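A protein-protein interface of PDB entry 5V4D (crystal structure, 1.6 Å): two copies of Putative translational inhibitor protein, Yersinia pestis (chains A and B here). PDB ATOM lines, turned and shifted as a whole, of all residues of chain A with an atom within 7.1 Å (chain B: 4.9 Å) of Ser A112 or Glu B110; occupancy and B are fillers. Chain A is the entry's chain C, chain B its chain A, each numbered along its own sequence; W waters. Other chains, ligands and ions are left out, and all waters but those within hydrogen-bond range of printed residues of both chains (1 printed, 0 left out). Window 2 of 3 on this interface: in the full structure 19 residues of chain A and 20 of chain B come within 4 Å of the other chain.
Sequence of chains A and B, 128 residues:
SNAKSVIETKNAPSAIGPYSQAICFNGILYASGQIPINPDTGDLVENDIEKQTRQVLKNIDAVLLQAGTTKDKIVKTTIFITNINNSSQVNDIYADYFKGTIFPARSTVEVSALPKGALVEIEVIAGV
O of Val B109 lies within hydrogen-bond range of N of Ile B81 (3.1 Å). OE1 of Glu B110 is in hydrogen-bond range of N of Ile B84 (2.8 Å). The backbone NH (N) of Val A111 is in hydrogen-bond range of the backbone carbonyl oxygen (O) of Ile A81.
Printed residues of chain B within 4 Å of Ser A112: Glu B110. Of chain A, only Val A111, Ser A112 and Ala A113 come within 4 Å of Glu B110. Of the printed residues of chain B, Glu A121 touches Thr B108 and Val B109. Of the printed residues of chain B, Pro A115 touches Ile B84 and Thr B108. Printed residues of chain B within 4 Å of Leu A114: Ile B84 and Val B109. Printed residues of chain A within 4 Å of Ile B84: Ala A113 (3.9 Å), Leu A114 (3.8 Å) and Pro A115 (3.9 Å). Of the printed residues of chain A, Val B109 touches Leu A114 and Glu A121. Ile B81 touches none of the printed residues of chain A. Thr A82 touches none of the printed residues of chain B. The nearest residue of chain B that does not touch Ser A112 is Val B111 (4.1 Å).
Water W1 lies within hydrogen-bond range of the backbone NH of Ser A112 (2.9 Å), the backbone carbonyl oxygen of Glu B110 (3.0 Å) and the backbone NH of Ser B112 (3.2 Å).
Among the printed residues, merely in contact across the chains: Val A111 with Glu B110 (3.2 Å), Ala A113 with Ile B84 (3.9 Å), Leu A114 with Ile B84 (3.8 Å), Leu A114 with Val B109 (3.8 Å), Pro A115 with Ile B84 (3.9 Å), Pro A115 with Thr B108 (3.4 Å) and Glu A121 with Val B109 (3.9 Å).
OG of Ser A112 lies within hydrogen-bond range of OE2 of Glu B110 (2.5 Å). The backbone carbonyl oxygen (O) of Ala A113 lies within hydrogen-bond range of the backbone NH (N) of Glu B110, at 3.1 Å. O of Thr B108 lies close to OE1 of Glu A121, at 3.0 Å.
Hydrophobic or aromatic side chains of chain B within 4 Å of the printed part of chain A: Ile B84 and Val B109. Hydrophobic or aromatic side chains of chain A that line the printed part of chain B: Val A111, Ala A113, Leu A114 and Pro A115. Among the printed residues, no Asp or Glu carboxylate lies within 4 Å of a Lys or Arg side-chain nitrogen of the other chain.
Val A111 touches Glu B110, but with the chains exchanged Glu A110 does not touch Val B111 (6.8 Å). Ser A112 touches Glu B110, but with the chains exchanged Glu A110 does not touch Ser B112 (6.7 Å). Positions printed for both chains: 81, 82, 110, 111 and 112.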
ATOM      1  N   ILE A  81      21.478 -16.143   9.581  1.00  0.00           N
ATOM      2  CA  ILE A  81      20.077 -16.545   9.481  1.00  0.00           C
ATOM      3  C   ILE A  81      19.375 -16.192  10.774  1.00  0.00           C
ATOM      4  O   ILE A  81      19.981 -16.207  11.845  1.00  0.00           O
ATOM      5  CB  ILE A  81      19.878 -18.044   9.178  1.00  0.00           C
ATOM      6  CG1 ILE A  81      20.697 -18.936  10.121  1.00  0.00           C
ATOM      7  CG2 ILE A  81      20.025 -18.303   7.645  1.00  0.00           C
ATOM      8  CD1 ILE A  81      20.617 -20.444   9.709  1.00  0.00           C
ATOM      9  N   THR A  82      18.065 -15.925  10.671  1.00  0.00           N
ATOM     10  CA  THR A  82      17.331 -15.606  11.891  1.00  0.00           C
ATOM     11  C   THR A  82      16.895 -16.837  12.647  1.00  0.00           C
ATOM     12  O   THR A  82      16.458 -16.700  13.808  1.00  0.00           O
ATOM     13  CB  THR A  82      16.094 -14.737  11.595  1.00  0.00           C
ATOM     14  OG1 THR A  82      15.204 -15.428  10.699  1.00  0.00           O
ATOM     15  CG2 THR A  82      16.504 -13.358  10.989  1.00  0.00           C
ATOM     16  N   GLU A 110      23.265 -17.734  13.843  1.00  0.00           N
ATOM     17  CA  GLU A 110      21.899 -17.256  13.971  1.00  0.00           C
ATOM     18  C   GLU A 110      21.912 -15.905  14.652  1.00  0.00           C
ATOM     19  O   GLU A 110      22.478 -15.762  15.738  1.00  0.00           O
ATOM     20  CB  GLU A 110      21.024 -18.221  14.781  1.00  0.00           C
ATOM     21  CG  GLU A 110      19.522 -17.755  14.833  1.00  0.00           C
ATOM     22  CD  GLU A 110      18.700 -18.471  15.936  1.00  0.00           C
ATOM     23  OE1 GLU A 110      18.202 -19.593  15.700  1.00  0.00           O
ATOM     24  OE2 GLU A 110      18.524 -17.899  17.042  1.00  0.00           O
ATOM     25  N   VAL A 111      21.270 -14.932  14.029  1.00  0.00           N
ATOM     26  CA  VAL A 111      21.124 -13.598  14.608  1.00  0.00           C
ATOM     27  C   VAL A 111      19.659 -13.375  14.916  1.00  0.00           C
ATOM     28  O   VAL A 111      18.789 -14.086  14.422  1.00  0.00           O
ATOM     29  CB  VAL A 111      21.654 -12.523  13.662  1.00  0.00           C
ATOM     30  CG1 VAL A 111      23.148 -12.705  13.514  1.00  0.00           C
ATOM     31  CG2 VAL A 111      20.932 -12.596  12.292  1.00  0.00           C
ATOM     32  N   SER A 112      19.369 -12.367  15.725  1.00  0.00           N
ATOM     33  CA  SER A 112      17.975 -12.249  16.116  1.00  0.00           C
ATOM     34  C   SER A 112      17.151 -11.437  15.126  1.00  0.00           C
ATOM     35  O   SER A 112      15.917 -11.526  15.143  1.00  0.00           O
ATOM     36  CB  SER A 112      17.862 -11.660  17.522  1.00  0.00           C
ATOM     37  OG  SER A 112      18.773 -10.627  17.687  1.00  0.00           O
ATOM     38  N   ALA A 113      17.793 -10.675  14.244  1.00  0.00           N
ATOM     39  CA  ALA A 113      17.065  -9.906  13.252  1.00  0.00           C
ATOM     40  C   ALA A 113      18.052  -9.483  12.171  1.00  0.00           C
ATOM     41  O   ALA A 113      19.267  -9.423  12.395  1.00  0.00           O
ATOM     42  CB  ALA A 113      16.396  -8.659  13.852  1.00  0.00           C
ATOM     43  N   LEU A 114      17.501  -9.168  11.002  1.00  0.00           N
ATOM     44  CA  LEU A 114      18.228  -8.759   9.813  1.00  0.00           C
ATOM     45  C   LEU A 114      17.521  -7.558   9.217  1.00  0.00           C
ATOM     46  O   LEU A 114      16.345  -7.320   9.507  1.00  0.00           O
ATOM     47  CB  LEU A 114      18.290  -9.890   8.768  1.00  0.00           C
ATOM     48  CG  LEU A 114      19.213 -11.051   9.199  1.00  0.00           C
ATOM     49  CD1 LEU A 114      19.078 -12.250   8.206  1.00  0.00           C
ATOM     50  CD2 LEU A 114      20.656 -10.618   9.269  1.00  0.00           C
ATOM     51  N   PRO A 115      18.199  -6.795   8.357  1.00  0.00           N
ATOM     52  CA  PRO A 115      17.536  -5.653   7.712  1.00  0.00           C
ATOM     53  C   PRO A 115      16.253  -6.074   7.002  1.00  0.00           C
ATOM     54  O   PRO A 115      16.175  -7.144   6.401  1.00  0.00           O
ATOM     55  CB  PRO A 115      18.587  -5.147   6.722  1.00  0.00           C
ATOM     56  CG  PRO A 115      19.893  -5.511   7.395  1.00  0.00           C
ATOM     57  CD  PRO A 115      19.621  -6.886   7.961  1.00  0.00           C
ATOM     58  N   ALA A 118      14.394  -9.638   6.901  1.00  0.00           N
ATOM     59  CA  ALA A 118      14.849 -10.791   6.140  1.00  0.00           C
ATOM     60  C   ALA A 118      15.107 -11.999   7.030  1.00  0.00           C
ATOM     61  O   ALA A 118      15.459 -11.868   8.211  1.00  0.00           O
ATOM     62  CB  ALA A 118      16.150 -10.450   5.414  1.00  0.00           C
ATOM     63  N   GLU A 121      20.788 -13.496   5.239  1.00  0.00           N
ATOM     64  CA  GLU A 121      21.671 -12.500   4.646  1.00  0.00           C
ATOM     65  C   GLU A 121      22.994 -13.198   4.367  1.00  0.00           C
ATOM     66  O   GLU A 121      23.541 -13.824   5.277  1.00  0.00           O
ATOM     67  CB  GLU A 121      21.898 -11.314   5.595  1.00  0.00           C
ATOM     68  CG  GLU A 121      22.881 -10.273   4.999  1.00  0.00           C
ATOM     69  CD  GLU A 121      23.074  -9.044   5.890  1.00  0.00           C
ATOM     70  OE1 GLU A 121      22.297  -8.837   6.871  1.00  0.00           O
ATOM     71  OE2 GLU A 121      24.038  -8.275   5.662  1.00  0.00           O
ATOM     72  N   ILE B  81      24.633  -4.542  15.751  1.00  0.00           N
ATOM     73  CA  ILE B  81      23.800  -3.696  16.594  1.00  0.00           C
ATOM     74  C   ILE B  81      22.881  -4.576  17.422  1.00  0.00           C
ATOM     75  O   ILE B  81      22.457  -5.645  16.987  1.00  0.00           O
ATOM     76  CB  ILE B  81      22.976  -2.654  15.800  1.00  0.00           C
ATOM     77  CG1 ILE B  81      22.293  -3.257  14.576  1.00  0.00           C
ATOM     78  CG2 ILE B  81      23.854  -1.488  15.413  1.00  0.00           C
ATOM     79  CD1 ILE B  81      21.275  -2.307  13.971  1.00  0.00           C
ATOM     80  N   THR B  82      22.560  -4.104  18.625  1.00  0.00           N
ATOM     81  CA  THR B  82      21.707  -4.913  19.494  1.00  0.00           C
ATOM     82  C   THR B  82      20.219  -4.752  19.186  1.00  0.00           C
ATOM     83  O   THR B  82      19.412  -5.544  19.683  1.00  0.00           O
ATOM     84  CB  THR B  82      21.950  -4.607  20.979  1.00  0.00           C
ATOM     85  OG1 THR B  82      21.668  -3.222  21.283  1.00  0.00           O
ATOM     86  CG2 THR B  82      23.377  -4.979  21.409  1.00  0.00           C
ATOM     87  N   ASN B  83      19.843  -3.775  18.359  1.00  0.00           N
ATOM     88  CA  ASN B  83      18.434  -3.532  18.047  1.00  0.00           C
ATOM     89  C   ASN B  83      18.408  -3.047  16.606  1.00  0.00           C
ATOM     90  O   ASN B  83      18.910  -1.953  16.311  1.00  0.00           O
ATOM     91  CB  ASN B  83      17.839  -2.491  18.986  1.00  0.00           C
ATOM     92  CG  ASN B  83      16.357  -2.229  18.716  1.00  0.00           C
ATOM     93  OD1 ASN B  83      15.796  -2.626  17.715  1.00  0.00           O
ATOM     94  ND2 ASN B  83      15.721  -1.534  19.652  1.00  0.00           N
ATOM     95  N   ILE B  84      17.875  -3.874  15.722  1.00  0.00           N
ATOM     96  CA  ILE B  84      17.820  -3.559  14.284  1.00  0.00           C
ATOM     97  C   ILE B  84      17.077  -2.258  14.037  1.00  0.00           C
ATOM     98  O   ILE B  84      17.327  -1.579  13.035  1.00  0.00           O
ATOM     99  CB  ILE B  84      17.193  -4.754  13.511  1.00  0.00           C
ATOM    100  CG1 ILE B  84      17.513  -4.714  12.025  1.00  0.00           C
ATOM    101  CG2 ILE B  84      15.678  -4.820  13.627  1.00  0.00           C
ATOM    102  CD1 ILE B  84      19.008  -4.961  11.736  1.00  0.00           C
ATOM    103  N   THR B 108      25.089  -5.572   7.986  1.00  0.00           N
ATOM    104  CA  THR B 108      24.486  -5.131   9.240  1.00  0.00           C
ATOM    105  C   THR B 108      23.673  -6.295   9.768  1.00  0.00           C
ATOM    106  O   THR B 108      22.851  -6.854   9.031  1.00  0.00           O
ATOM    107  CB  THR B 108      23.550  -3.924   9.042  1.00  0.00           C
ATOM    108  OG1 THR B 108      24.295  -2.837   8.488  1.00  0.00           O
ATOM    109  CG2 THR B 108      22.921  -3.505  10.430  1.00  0.00           C
ATOM    110  N   VAL B 109      23.882  -6.651  11.031  1.00  0.00           N
ATOM    111  CA  VAL B 109      23.109  -7.730  11.655  1.00  0.00           C
ATOM    112  C   VAL B 109      22.759  -7.343  13.082  1.00  0.00           C
ATOM    113  O   VAL B 109      23.489  -6.591  13.731  1.00  0.00           O
ATOM    114  CB  VAL B 109      23.878  -9.087  11.664  1.00  0.00           C
ATOM    115  CG1 VAL B 109      24.150  -9.566  10.208  1.00  0.00           C
ATOM    116  CG2 VAL B 109      25.180  -9.027  12.451  1.00  0.00           C
ATOM    117  N   GLU B 110      21.634  -7.867  13.587  1.00  0.00           N
ATOM    118  CA  GLU B 110      21.284  -7.680  14.991  1.00  0.00           C
ATOM    119  C   GLU B 110      21.888  -8.793  15.840  1.00  0.00           C
ATOM    120  O   GLU B 110      21.566  -9.969  15.658  1.00  0.00           O
ATOM    121  CB  GLU B 110      19.770  -7.641  15.181  1.00  0.00           C
ATOM    122  CG  GLU B 110      19.402  -7.215  16.624  1.00  0.00           C
ATOM    123  CD  GLU B 110      17.914  -7.366  16.864  1.00  0.00           C
ATOM    124  OE1 GLU B 110      17.138  -6.423  16.605  1.00  0.00           O
ATOM    125  OE2 GLU B 110      17.500  -8.475  17.288  1.00  0.00           O
ATOM    126  N   VAL B 111      22.741  -8.423  16.759  1.00  0.00           N
ATOM    127  CA  VAL B 111      23.339  -9.360  17.711  1.00  0.00           C
ATOM    128  C   VAL B 111      22.571  -9.296  19.029  1.00  0.00           C
ATOM    129  O   VAL B 111      21.798  -8.361  19.301  1.00  0.00           O
ATOM    130  CB  VAL B 111      24.821  -9.041  17.946  1.00  0.00           C
ATOM    131  CG1 VAL B 111      25.586  -9.165  16.619  1.00  0.00           C
ATOM    132  CG2 VAL B 111      24.999  -7.636  18.511  1.00  0.00           C
ATOM    133  N   SER B 112      22.764 -10.306  19.875  1.00  0.00           N
ATOM    134  CA  SER B 112      21.992 -10.225  21.107  1.00  0.00           C
ATOM    135  C   SER B 112      22.696  -9.370  22.159  1.00  0.00           C
ATOM    136  O   SER B 112      22.022  -8.652  22.919  1.00  0.00           O
ATOM    137  CB  SER B 112      21.631 -11.628  21.637  1.00  0.00           C
ATOM    138  OG  SER B 112      22.705 -12.538  21.651  1.00  0.00           O
HETATM  139  O   HOH W   1      21.563 -12.225  17.559  1.00  0.00           O
